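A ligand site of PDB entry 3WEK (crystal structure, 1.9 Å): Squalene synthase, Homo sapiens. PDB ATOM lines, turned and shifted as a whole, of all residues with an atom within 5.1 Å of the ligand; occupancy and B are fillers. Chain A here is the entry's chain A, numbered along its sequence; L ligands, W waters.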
ATOM      1  N   THR A  23     -27.987 -17.165  32.246  1.00  0.00           N
ATOM      2  CA  THR A  23     -27.615 -16.299  31.125  1.00  0.00           C
ATOM      3  C   THR A  23     -27.562 -16.926  29.732  1.00  0.00           C
ATOM      4  O   THR A  23     -27.397 -16.202  28.753  1.00  0.00           O
ATOM      5  CB  THR A  23     -26.277 -15.559  31.386  1.00  0.00           C
ATOM      6  OG1 THR A  23     -25.210 -16.521  31.506  1.00  0.00           O
ATOM      7  CG2 THR A  23     -26.352 -14.721  32.660  1.00  0.00           C
ATOM      8  N   SER A  24     -27.670 -18.241  29.626  1.00  0.00           N
ATOM      9  CA  SER A  24     -27.528 -18.895  28.327  1.00  0.00           C
ATOM     10  C   SER A  24     -28.734 -19.727  27.922  1.00  0.00           C
ATOM     11  O   SER A  24     -28.902 -20.864  28.370  1.00  0.00           O
ATOM     12  CB  SER A  24     -26.264 -19.745  28.246  1.00  0.00           C
ATOM     13  OG  SER A  24     -26.070 -20.186  26.917  1.00  0.00           O
ATOM     14  N   ARG A  25     -29.556 -19.142  27.052  1.00  0.00           N
ATOM     15  CA  ARG A  25     -30.728 -19.780  26.473  1.00  0.00           C
ATOM     16  C   ARG A  25     -30.346 -20.847  25.449  1.00  0.00           C
ATOM     17  O   ARG A  25     -31.057 -21.840  25.288  1.00  0.00           O
ATOM     18  CB  ARG A  25     -31.584 -18.719  25.785  1.00  0.00           C
ATOM     19  CG  ARG A  25     -32.278 -17.755  26.732  1.00  0.00           C
ATOM     20  CD  ARG A  25     -32.841 -16.568  25.957  1.00  0.00           C
ATOM     21  NE  ARG A  25     -34.249 -16.320  26.285  1.00  0.00           N
ATOM     22  CZ  ARG A  25     -35.136 -15.828  25.428  1.00  0.00           C
ATOM     23  NH1 ARG A  25     -34.781 -15.542  24.177  1.00  0.00           N
ATOM     24  NH2 ARG A  25     -36.394 -15.644  25.807  1.00  0.00           N
ATOM     25  N   SER A  26     -29.221 -20.643  24.767  1.00  0.00           N
ATOM     26  CA  SER A  26     -28.754 -21.475  23.658  1.00  0.00           C
ATOM     27  C   SER A  26     -27.768 -22.585  24.000  1.00  0.00           C
ATOM     28  O   SER A  26     -27.663 -23.559  23.248  1.00  0.00           O
ATOM     29  CB  SER A  26     -28.114 -20.617  22.567  1.00  0.00           C
ATOM     30  OG  SER A  26     -29.045 -20.235  21.577  1.00  0.00           O
ATOM     31  N   PHE A  27     -27.011 -22.455  25.084  1.00  0.00           N
ATOM     32  CA  PHE A  27     -25.872 -23.345  25.294  1.00  0.00           C
ATOM     33  C   PHE A  27     -25.834 -24.105  26.615  1.00  0.00           C
ATOM     34  O   PHE A  27     -24.939 -24.936  26.808  1.00  0.00           O
ATOM     35  CB  PHE A  27     -24.546 -22.579  25.122  1.00  0.00           C
ATOM     36  CG  PHE A  27     -24.425 -21.783  23.861  1.00  0.00           C
ATOM     37  CD1 PHE A  27     -24.292 -22.398  22.629  1.00  0.00           C
ATOM     38  CD2 PHE A  27     -24.386 -20.390  23.907  1.00  0.00           C
ATOM     39  CE1 PHE A  27     -24.175 -21.654  21.465  1.00  0.00           C
ATOM     40  CE2 PHE A  27     -24.247 -19.634  22.745  1.00  0.00           C
ATOM     41  CZ  PHE A  27     -24.154 -20.272  21.519  1.00  0.00           C
ATOM     42  N   ILE A  31     -23.603 -27.612  27.151  1.00  0.00           N
ATOM     43  CA  ILE A  31     -22.363 -27.414  27.876  1.00  0.00           C
ATOM     44  C   ILE A  31     -22.273 -28.379  29.050  1.00  0.00           C
ATOM     45  O   ILE A  31     -21.253 -29.005  29.292  1.00  0.00           O
ATOM     46  CB  ILE A  31     -22.205 -25.921  28.316  1.00  0.00           C
ATOM     47  CG1 ILE A  31     -21.713 -25.088  27.141  1.00  0.00           C
ATOM     48  CG2 ILE A  31     -21.219 -25.772  29.475  1.00  0.00           C
ATOM     49  CD1 ILE A  31     -21.819 -23.595  27.358  1.00  0.00           C
ATOM     50  N   VAL A  42     -15.371 -25.250  29.286  1.00  0.00           N
ATOM     51  CA  VAL A  42     -16.295 -24.550  28.389  1.00  0.00           C
ATOM     52  C   VAL A  42     -17.302 -23.668  29.143  1.00  0.00           C
ATOM     53  O   VAL A  42     -17.598 -22.563  28.674  1.00  0.00           O
ATOM     54  CB  VAL A  42     -17.006 -25.509  27.396  1.00  0.00           C
ATOM     55  CG1 VAL A  42     -17.952 -24.759  26.475  1.00  0.00           C
ATOM     56  CG2 VAL A  42     -15.958 -26.248  26.573  1.00  0.00           C
ATOM     57  N   PHE A  45     -15.392 -20.647  30.008  1.00  0.00           N
ATOM     58  CA  PHE A  45     -15.121 -19.924  28.766  1.00  0.00           C
ATOM     59  C   PHE A  45     -16.333 -19.065  28.413  1.00  0.00           C
ATOM     60  O   PHE A  45     -16.192 -17.853  28.187  1.00  0.00           O
ATOM     61  CB  PHE A  45     -14.790 -20.902  27.644  1.00  0.00           C
ATOM     62  CG  PHE A  45     -14.297 -20.258  26.384  1.00  0.00           C
ATOM     63  CD1 PHE A  45     -13.522 -19.101  26.425  1.00  0.00           C
ATOM     64  CD2 PHE A  45     -14.607 -20.825  25.145  1.00  0.00           C
ATOM     65  CE1 PHE A  45     -13.055 -18.510  25.260  1.00  0.00           C
ATOM     66  CE2 PHE A  45     -14.153 -20.244  23.974  1.00  0.00           C
ATOM     67  CZ  PHE A  45     -13.375 -19.077  24.025  1.00  0.00           C
ATOM     68  N   TYR A  46     -17.503 -19.691  28.420  1.00  0.00           N
ATOM     69  CA  TYR A  46     -18.780 -18.999  28.272  1.00  0.00           C
ATOM     70  C   TYR A  46     -18.923 -17.788  29.186  1.00  0.00           C
ATOM     71  O   TYR A  46     -19.322 -16.709  28.723  1.00  0.00           O
ATOM     72  CB  TYR A  46     -19.957 -19.940  28.560  1.00  0.00           C
ATOM     73  CG  TYR A  46     -21.275 -19.201  28.480  1.00  0.00           C
ATOM     74  CD1 TYR A  46     -21.883 -18.980  27.244  1.00  0.00           C
ATOM     75  CD2 TYR A  46     -21.884 -18.687  29.621  1.00  0.00           C
ATOM     76  CE1 TYR A  46     -23.076 -18.275  27.150  1.00  0.00           C
ATOM     77  CE2 TYR A  46     -23.092 -17.992  29.543  1.00  0.00           C
ATOM     78  CZ  TYR A  46     -23.671 -17.790  28.296  1.00  0.00           C
ATOM     79  OH  TYR A  46     -24.851 -17.094  28.177  1.00  0.00           O
ATOM     80  N   LEU A  49     -16.578 -14.803  28.537  1.00  0.00           N
ATOM     81  CA  LEU A  49     -16.958 -14.102  27.322  1.00  0.00           C
ATOM     82  C   LEU A  49     -18.276 -13.376  27.498  1.00  0.00           C
ATOM     83  O   LEU A  49     -18.454 -12.285  26.943  1.00  0.00           O
ATOM     84  CB  LEU A  49     -16.971 -15.075  26.135  1.00  0.00           C
ATOM     85  CG  LEU A  49     -15.594 -15.604  25.712  1.00  0.00           C
ATOM     86  CD1 LEU A  49     -15.746 -16.392  24.437  1.00  0.00           C
ATOM     87  CD2 LEU A  49     -14.499 -14.558  25.561  1.00  0.00           C
ATOM     88  N   ARG A  50     -19.200 -13.952  28.267  1.00  0.00           N
ATOM     89  CA  ARG A  50     -20.427 -13.245  28.601  1.00  0.00           C
ATOM     90  C   ARG A  50     -20.135 -11.952  29.376  1.00  0.00           C
ATOM     91  O   ARG A  50     -20.723 -10.914  29.090  1.00  0.00           O
ATOM     92  CB  ARG A  50     -21.397 -14.184  29.335  1.00  0.00           C
ATOM     93  CG  ARG A  50     -22.704 -13.562  29.817  1.00  0.00           C
ATOM     94  CD  ARG A  50     -23.438 -12.879  28.679  1.00  0.00           C
ATOM     95  NE  ARG A  50     -24.016 -13.813  27.733  1.00  0.00           N
ATOM     96  CZ  ARG A  50     -24.347 -13.489  26.479  1.00  0.00           C
ATOM     97  NH1 ARG A  50     -24.139 -12.251  26.037  1.00  0.00           N
ATOM     98  NH2 ARG A  50     -24.902 -14.394  25.684  1.00  0.00           N
ATOM     99  N   ASP A  53     -18.628  -9.380  26.980  1.00  0.00           N
ATOM    100  CA  ASP A  53     -19.684  -8.866  26.100  1.00  0.00           C
ATOM    101  C   ASP A  53     -20.593  -7.879  26.818  1.00  0.00           C
ATOM    102  O   ASP A  53     -21.073  -6.921  26.204  1.00  0.00           O
ATOM    103  CB  ASP A  53     -20.542  -9.999  25.524  1.00  0.00           C
ATOM    104  CG  ASP A  53     -21.394  -9.521  24.356  1.00  0.00           C
ATOM    105  OD1 ASP A  53     -20.815  -8.948  23.405  1.00  0.00           O
ATOM    106  OD2 ASP A  53     -22.629  -9.690  24.397  1.00  0.00           O
ATOM    107  N   MET A 123     -10.222 -10.928  21.542  1.00  0.00           N
ATOM    108  CA  MET A 123     -11.556 -10.399  21.416  1.00  0.00           C
ATOM    109  C   MET A 123     -11.629  -8.949  21.919  1.00  0.00           C
ATOM    110  O   MET A 123     -12.213  -8.095  21.270  1.00  0.00           O
ATOM    111  CB  MET A 123     -12.564 -11.289  22.142  1.00  0.00           C
ATOM    112  CG  MET A 123     -13.982 -10.814  22.014  1.00  0.00           C
ATOM    113  SD  MET A 123     -15.218 -11.964  22.634  1.00  0.00           S
ATOM    114  CE  MET A 123     -14.672 -13.488  21.870  1.00  0.00           C
ATOM    115  N   MET A 127     -13.013  -5.878  19.801  1.00  0.00           N
ATOM    116  CA  MET A 127     -14.187  -5.109  20.202  1.00  0.00           C
ATOM    117  C   MET A 127     -13.861  -3.614  20.376  1.00  0.00           C
ATOM    118  O   MET A 127     -14.643  -2.754  19.971  1.00  0.00           O
ATOM    119  CB  MET A 127     -14.740  -5.646  21.516  1.00  0.00           C
ATOM    120  CG  MET A 127     -15.505  -6.942  21.396  1.00  0.00           C
ATOM    121  SD  MET A 127     -15.625  -7.634  23.052  1.00  0.00           S
ATOM    122  CE  MET A 127     -17.134  -8.565  22.908  1.00  0.00           C
ATOM    123  N   VAL A 148     -16.004 -11.163  17.592  1.00  0.00           N
ATOM    124  CA  VAL A 148     -17.000 -11.506  18.600  1.00  0.00           C
ATOM    125  C   VAL A 148     -17.566 -12.934  18.567  1.00  0.00           C
ATOM    126  O   VAL A 148     -18.296 -13.343  19.478  1.00  0.00           O
ATOM    127  CB  VAL A 148     -18.172 -10.471  18.669  1.00  0.00           C
ATOM    128  CG1 VAL A 148     -17.627  -9.046  18.848  1.00  0.00           C
ATOM    129  CG2 VAL A 148     -19.067 -10.545  17.422  1.00  0.00           C
ATOM    130  N   ALA A 149     -17.262 -13.694  17.518  1.00  0.00           N
ATOM    131  CA  ALA A 149     -17.897 -14.993  17.319  1.00  0.00           C
ATOM    132  C   ALA A 149     -16.931 -15.989  16.697  1.00  0.00           C
ATOM    133  O   ALA A 149     -16.827 -17.132  17.131  1.00  0.00           O
ATOM    134  CB  ALA A 149     -19.108 -14.827  16.433  1.00  0.00           C
ATOM    135  N   VAL A 152     -14.620 -17.259  19.215  1.00  0.00           N
ATOM    136  CA  VAL A 152     -15.219 -18.223  20.110  1.00  0.00           C
ATOM    137  C   VAL A 152     -15.082 -19.650  19.583  1.00  0.00           C
ATOM    138  O   VAL A 152     -14.587 -20.538  20.276  1.00  0.00           O
ATOM    139  CB  VAL A 152     -16.681 -17.886  20.394  1.00  0.00           C
ATOM    140  CG1 VAL A 152     -17.178 -18.817  21.454  1.00  0.00           C
ATOM    141  CG2 VAL A 152     -16.818 -16.407  20.782  1.00  0.00           C
ATOM    142  N   GLY A 153     -15.433 -19.847  18.316  1.00  0.00           N
ATOM    143  CA  GLY A 153     -15.280 -21.152  17.676  1.00  0.00           C
ATOM    144  C   GLY A 153     -13.821 -21.572  17.607  1.00  0.00           C
ATOM    145  O   GLY A 153     -13.504 -22.752  17.802  1.00  0.00           O
ATOM    146  N   ILE A 154     -12.943 -20.596  17.408  1.00  0.00           N
ATOM    147  CA  ILE A 154     -11.509 -20.898  17.402  1.00  0.00           C
ATOM    148  C   ILE A 154     -11.054 -21.339  18.802  1.00  0.00           C
ATOM    149  O   ILE A 154     -10.348 -22.349  18.948  1.00  0.00           O
ATOM    150  CB  ILE A 154     -10.657 -19.758  16.839  1.00  0.00           C
ATOM    151  CG1 ILE A 154     -10.779 -19.700  15.306  1.00  0.00           C
ATOM    152  CG2 ILE A 154      -9.162 -19.942  17.161  1.00  0.00           C
ATOM    153  CD1 ILE A 154     -10.358 -18.349  14.732  1.00  0.00           C
ATOM    154  N   LEU A 156     -13.114 -22.537  21.314  1.00  0.00           N
ATOM    155  CA  LEU A 156     -13.776 -23.804  21.593  1.00  0.00           C
ATOM    156  C   LEU A 156     -12.974 -24.948  21.001  1.00  0.00           C
ATOM    157  O   LEU A 156     -12.754 -25.960  21.679  1.00  0.00           O
ATOM    158  CB  LEU A 156     -15.203 -23.874  21.044  1.00  0.00           C
ATOM    159  CG  LEU A 156     -16.187 -23.113  21.928  1.00  0.00           C
ATOM    160  CD1 LEU A 156     -17.523 -23.005  21.217  1.00  0.00           C
ATOM    161  CD2 LEU A 156     -16.329 -23.792  23.293  1.00  0.00           C
ATOM    162  N   SER A 157     -12.525 -24.768  19.757  1.00  0.00           N
ATOM    163  CA  SER A 157     -11.793 -25.793  19.020  1.00  0.00           C
ATOM    164  C   SER A 157     -10.435 -26.078  19.649  1.00  0.00           C
ATOM    165  O   SER A 157     -10.005 -27.230  19.663  1.00  0.00           O
ATOM    166  CB  SER A 157     -11.576 -25.399  17.553  1.00  0.00           C
ATOM    167  OG  SER A 157     -12.785 -25.066  16.901  1.00  0.00           O
ATOM    168  N   PHE A 160     -11.244 -28.207  22.756  1.00  0.00           N
ATOM    169  CA  PHE A 160     -11.458 -29.582  22.295  1.00  0.00           C
ATOM    170  C   PHE A 160     -10.098 -30.264  22.007  1.00  0.00           C
ATOM    171  O   PHE A 160      -9.836 -31.360  22.499  1.00  0.00           O
ATOM    172  CB  PHE A 160     -12.304 -29.573  21.019  1.00  0.00           C
ATOM    173  CG  PHE A 160     -13.655 -28.928  21.154  1.00  0.00           C
ATOM    174  CD1 PHE A 160     -14.328 -28.939  22.363  1.00  0.00           C
ATOM    175  CD2 PHE A 160     -14.276 -28.340  20.050  1.00  0.00           C
ATOM    176  CE1 PHE A 160     -15.610 -28.371  22.472  1.00  0.00           C
ATOM    177  CE2 PHE A 160     -15.535 -27.761  20.162  1.00  0.00           C
ATOM    178  CZ  PHE A 160     -16.209 -27.771  21.371  1.00  0.00           C
ATOM    179  N   ALA A 177     -13.229 -23.341  12.051  1.00  0.00           N
ATOM    180  CA  ALA A 177     -13.754 -22.885  13.353  1.00  0.00           C
ATOM    181  C   ALA A 177     -14.303 -21.458  13.286  1.00  0.00           C
ATOM    182  O   ALA A 177     -15.364 -21.157  13.837  1.00  0.00           O
ATOM    183  CB  ALA A 177     -12.664 -22.990  14.411  1.00  0.00           C
ATOM    184  N   MET A 180     -17.655 -21.403  11.678  1.00  0.00           N
ATOM    185  CA  MET A 180     -18.656 -21.875  12.625  1.00  0.00           C
ATOM    186  C   MET A 180     -19.171 -20.701  13.452  1.00  0.00           C
ATOM    187  O   MET A 180     -20.381 -20.583  13.718  1.00  0.00           O
ATOM    188  CB  MET A 180     -18.052 -22.972  13.523  1.00  0.00           C
ATOM    189  CG  MET A 180     -17.802 -24.341  12.848  1.00  0.00           C
ATOM    190  SD  MET A 180     -19.352 -25.287  12.879  1.00  0.00           S
ATOM    191  CE  MET A 180     -19.404 -25.756  14.605  1.00  0.00           C
ATOM    192  N   GLY A 181     -18.237 -19.842  13.851  1.00  0.00           N
ATOM    193  CA  GLY A 181     -18.564 -18.638  14.641  1.00  0.00           C
ATOM    194  C   GLY A 181     -19.317 -17.620  13.819  1.00  0.00           C
ATOM    195  O   GLY A 181     -20.416 -17.168  14.203  1.00  0.00           O
ATOM    196  N   LEU A 184     -23.166 -18.312  13.068  1.00  0.00           N
ATOM    197  CA  LEU A 184     -24.218 -18.078  14.096  1.00  0.00           C
ATOM    198  C   LEU A 184     -24.426 -16.569  14.329  1.00  0.00           C
ATOM    199  O   LEU A 184     -25.527 -16.096  14.682  1.00  0.00           O
ATOM    200  CB  LEU A 184     -23.787 -18.709  15.431  1.00  0.00           C
ATOM    201  CG  LEU A 184     -23.622 -20.224  15.544  1.00  0.00           C
ATOM    202  CD1 LEU A 184     -23.139 -20.554  16.976  1.00  0.00           C
ATOM    203  CD2 LEU A 184     -24.938 -20.933  15.232  1.00  0.00           C
ATOM    204  N   GLN A 185     -23.335 -15.834  14.181  1.00  0.00           N
ATOM    205  CA  GLN A 185     -23.300 -14.405  14.453  1.00  0.00           C
ATOM    206  C   GLN A 185     -23.990 -13.639  13.331  1.00  0.00           C
ATOM    207  O   GLN A 185     -24.817 -12.782  13.613  1.00  0.00           O
ATOM    208  CB  GLN A 185     -21.851 -13.908  14.631  1.00  0.00           C
ATOM    209  CG  GLN A 185     -21.749 -12.408  15.037  1.00  0.00           C
ATOM    210  CD  GLN A 185     -22.311 -12.115  16.417  1.00  0.00           C
ATOM    211  OE1 GLN A 185     -21.605 -12.237  17.414  1.00  0.00           O
ATOM    212  NE2 GLN A 185     -23.593 -11.757  16.495  1.00  0.00           N
ATOM    213  N   ASN A 188     -27.672 -14.183  13.861  1.00  0.00           N
ATOM    214  CA  ASN A 188     -28.311 -13.379  14.905  1.00  0.00           C
ATOM    215  C   ASN A 188     -28.430 -11.916  14.477  1.00  0.00           C
ATOM    216  O   ASN A 188     -29.470 -11.288  14.700  1.00  0.00           O
ATOM    217  CB  ASN A 188     -27.590 -13.506  16.260  1.00  0.00           C
ATOM    218  CG  ASN A 188     -27.555 -14.944  16.783  1.00  0.00           C
ATOM    219  OD1 ASN A 188     -27.962 -15.884  16.093  1.00  0.00           O
ATOM    220  ND2 ASN A 188     -27.033 -15.118  17.998  1.00  0.00           N
ATOM    221  N   ARG A 191     -31.244 -11.652  12.041  1.00  0.00           N
ATOM    222  CA  ARG A 191     -32.518 -11.834  12.757  1.00  0.00           C
ATOM    223  C   ARG A 191     -32.873 -10.643  13.643  1.00  0.00           C
ATOM    224  O   ARG A 191     -34.042 -10.342  13.903  1.00  0.00           O
ATOM    225  CB  ARG A 191     -32.464 -13.067  13.678  1.00  0.00           C
ATOM    226  CG  ARG A 191     -33.793 -13.411  14.394  1.00  0.00           C
ATOM    227  CD  ARG A 191     -33.619 -14.293  15.632  1.00  0.00           C
ATOM    228  NE  ARG A 191     -32.624 -13.709  16.532  1.00  0.00           N
ATOM    229  CZ  ARG A 191     -31.842 -14.386  17.364  1.00  0.00           C
ATOM    230  NH1 ARG A 191     -31.947 -15.704  17.469  1.00  0.00           N
ATOM    231  NH2 ARG A 191     -30.945 -13.724  18.097  1.00  0.00           N
ATOM    232  N   TYR A 249     -16.236 -28.968   9.315  1.00  0.00           N
ATOM    233  CA  TYR A 249     -16.026 -28.991  10.773  1.00  0.00           C
ATOM    234  C   TYR A 249     -16.827 -30.072  11.540  1.00  0.00           C
ATOM    235  O   TYR A 249     -16.262 -30.858  12.292  1.00  0.00           O
ATOM    236  CB  TYR A 249     -16.362 -27.604  11.363  1.00  0.00           C
ATOM    237  CG  TYR A 249     -15.926 -27.435  12.800  1.00  0.00           C
ATOM    238  CD1 TYR A 249     -16.781 -27.802  13.842  1.00  0.00           C
ATOM    239  CD2 TYR A 249     -14.664 -26.920  13.111  1.00  0.00           C
ATOM    240  CE1 TYR A 249     -16.373 -27.683  15.163  1.00  0.00           C
ATOM    241  CE2 TYR A 249     -14.261 -26.780  14.423  1.00  0.00           C
ATOM    242  CZ  TYR A 249     -15.136 -27.158  15.440  1.00  0.00           C
ATOM    243  OH  TYR A 249     -14.751 -27.040  16.758  1.00  0.00           O
ATOM    244  N   CYS A 262     -21.476 -28.610  19.246  1.00  0.00           N
ATOM    245  CA  CYS A 262     -21.255 -27.919  17.980  1.00  0.00           C
ATOM    246  C   CYS A 262     -22.407 -27.999  16.988  1.00  0.00           C
ATOM    247  O   CYS A 262     -22.720 -26.992  16.344  1.00  0.00           O
ATOM    248  CB  CYS A 262     -19.969 -28.418  17.314  1.00  0.00           C
ATOM    249  SG  CYS A 262     -18.578 -28.229  18.420  1.00  0.00           S
ATOM    250  N   GLN A 266     -25.706 -24.846  15.332  1.00  0.00           N
ATOM    251  CA  GLN A 266     -25.612 -24.609  13.889  1.00  0.00           C
ATOM    252  C   GLN A 266     -26.948 -24.862  13.211  1.00  0.00           C
ATOM    253  O   GLN A 266     -27.358 -24.107  12.327  1.00  0.00           O
ATOM    254  CB  GLN A 266     -24.553 -25.459  13.223  1.00  0.00           C
ATOM    255  CG  GLN A 266     -23.102 -25.136  13.614  1.00  0.00           C
ATOM    256  CD  GLN A 266     -22.700 -23.682  13.409  1.00  0.00           C
ATOM    257  OE1 GLN A 266     -22.145 -23.039  14.311  1.00  0.00           O
ATOM    258  NE2 GLN A 266     -22.969 -23.146  12.238  1.00  0.00           N
HETATM  259  C1  LIG L   1     -20.300 -21.717  23.882  1.00  0.00           C
HETATM  260  C2  LIG L   1     -18.034 -20.571  24.748  1.00  0.00           C
HETATM  261  C3  LIG L   1     -16.370 -24.203  16.742  1.00  0.00           C
HETATM  262  C4  LIG L   1     -18.703 -24.613  17.968  1.00  0.00           C
HETATM  263  C5  LIG L   1     -20.866 -15.188  25.314  1.00  0.00           C
HETATM  264  C6  LIG L   1     -20.729 -20.506  20.008  1.00  0.00           C
HETATM  265  C7  LIG L   1     -22.153 -12.696  22.767  1.00  0.00           C
HETATM  266  C8  LIG L   1     -23.590 -15.669  18.251  1.00  0.00           C
HETATM  267  O1  LIG L   1     -28.347 -18.280  24.844  1.00  0.00           O
HETATM  268  O2  LIG L   1     -27.804 -17.802  20.836  1.00  0.00           O
HETATM  269  O3  LIG L   1     -28.263 -15.744  24.946  1.00  0.00           O
HETATM  270  O4  LIG L   1     -29.421 -16.880  22.978  1.00  0.00           O
HETATM  271  O5  LIG L   1     -27.528 -15.355  21.475  1.00  0.00           O
HETATM  272  C9  LIG L   1     -20.041 -19.234  24.016  1.00  0.00           C
HETATM  273  C10 LIG L   1     -18.018 -22.334  17.059  1.00  0.00           C
HETATM  274  C11 LIG L   1     -19.409 -14.665  23.207  1.00  0.00           C
HETATM  275  C12 LIG L   1     -20.204 -18.410  18.786  1.00  0.00           C
HETATM  276  C13 LIG L   1     -21.247 -13.691  20.601  1.00  0.00           C
HETATM  277  C14 LIG L   1     -19.519 -17.970  24.225  1.00  0.00           C
HETATM  278  C15 LIG L   1     -19.137 -21.602  17.429  1.00  0.00           C
HETATM  279  C16 LIG L   1     -19.090 -13.321  23.342  1.00  0.00           C
HETATM  280  C17 LIG L   1     -21.253 -17.759  19.450  1.00  0.00           C
HETATM  281  C18 LIG L   1     -20.365 -16.958  23.469  1.00  0.00           C
HETATM  282  C19 LIG L   1     -18.701 -20.403  18.289  1.00  0.00           C
HETATM  283  C20 LIG L   1     -19.614 -12.486  22.159  1.00  0.00           C
HETATM  284  C21 LIG L   1     -24.728 -15.494  20.942  1.00  0.00           C
HETATM  285  C22 LIG L   1     -21.237 -16.243  19.249  1.00  0.00           C
HETATM  286  O6  LIG L   1     -25.385 -16.777  20.974  1.00  0.00           O
HETATM  287  O7  LIG L   1     -26.859 -17.081  23.151  1.00  0.00           O
HETATM  288  C23 LIG L   1     -19.478 -20.472  24.236  1.00  0.00           C
HETATM  289  C24 LIG L   1     -17.712 -23.684  17.258  1.00  0.00           C
HETATM  290  C25 LIG L   1     -20.185 -15.535  23.986  1.00  0.00           C
HETATM  291  C26 LIG L   1     -19.879 -19.739  19.010  1.00  0.00           C
HETATM  292  C27 LIG L   1     -21.022 -12.968  21.774  1.00  0.00           C
HETATM  293  C28 LIG L   1     -22.628 -14.231  20.164  1.00  0.00           C
HETATM  294  C29 LIG L   1     -23.189 -15.499  20.832  1.00  0.00           C
HETATM  295  C30 LIG L   1     -22.607 -15.560  19.423  1.00  0.00           C
HETATM  296  P1  LIG L   1     -28.204 -16.909  24.042  1.00  0.00           P
HETATM  297  P2  LIG L   1     -26.918 -16.849  21.552  1.00  0.00           P
HETATM  298  O   HOH W   1     -26.359 -12.320  22.359  1.00  0.00           O
HETATM  299  O   HOH W   2     -21.938 -24.431  16.924  1.00  0.00           O
HETATM  300  O   HOH W   3     -26.750 -19.004  18.317  1.00  0.00           O
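N of Ser 26 lies within hydrogen-bond range of O1 of the ligand, 2.5 Å away.
O1 of the ligand is in hydrogen-bond range of N of Arg 25, 2.7 Å away.
OG of Ser 26 is in hydrogen-bond range of O2 of the ligand.
O3 of the ligand is in salt-bridge range of NH2 of Arg 50, at 3.7 Å.
The backbone NH (N) of Phe 27 lies within hydrogen-bond range of the side-chain hydroxyl (OG) of Ser 24 (3.1 Å).
The side-chain amide oxygen of Gln 266 sits close to the backbone carbonyl oxygen of Met 180, at 3.1 Å.
The side-chain hydroxyl of Tyr 46 lies within hydrogen-bond range of the backbone carbonyl oxygen of Thr 23 (2.8 Å).
The side-chain amide oxygen (OD1) of Asn 188 lies close to the backbone carbonyl oxygen (O) of Leu 184 (2.8 Å).
OD2 of Asp 53 is in salt-bridge range of NH1 of Arg 50, at 3.4 Å.
OH of Tyr 249 lies within hydrogen-bond range of OG of Ser 157, 2.8 Å away.
OG of Ser 157 sits at hydrogen-bond distance from O of Gly 153 (2.6 Å).
N of Ser 24 lies close to OH of Tyr 46, 3.4 Å away.
Thr 23 touches the ligand (O to O3, 3.9 Å).
Ser 24 touches the ligand (C to O1, 3.4 Å).
Phe 27 touches the ligand (CE2 to O6, 3.5 Å).
Phe 45 touches the ligand.
Tyr 46 touches the ligand.
Leu 49 touches the ligand (O to C16, 3.8 Å).
OD2 of Asp 53 touches C7 of the ligand, at 3.5 Å.
Val 148 touches the ligand (O to C20, 3.1 Å).
Ala 149 touches the ligand (CB to C22, 3.8 Å).
CG1 of Val 152 touches C14 of the ligand (3.7 Å).
CA of Gly 153 touches C10 of the ligand, 3.0 Å away.
CD1 of Leu 156 touches C4 of the ligand, 3.8 Å away.
OG of Ser 157 touches C3 of the ligand, at 3.7 Å.
Met 180 touches the ligand.
Leu 184 touches the ligand.
Gln 185 touches the ligand (OE1 to C13, 3.5 Å).
ND2 of Asn 188 touches C8 of the ligand (3.5 Å).
Tyr 249 touches the ligand.
Cys 262 touches the ligand.
Hydrophobic or aromatic side chains within 4 Å of the ligand: Phe 27, Phe 45, Tyr 46, Leu 49, Ala 149, Val 152, Leu 156, Met 180, Leu 184 and Tyr 249.
Of the 32 residues printed, 22 come within 4 Å of the ligand.
Water W2 bridges the backbone carbonyl oxygen (O) of Cys 262 and the side-chain amide oxygen (OE1) of Gln 266.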
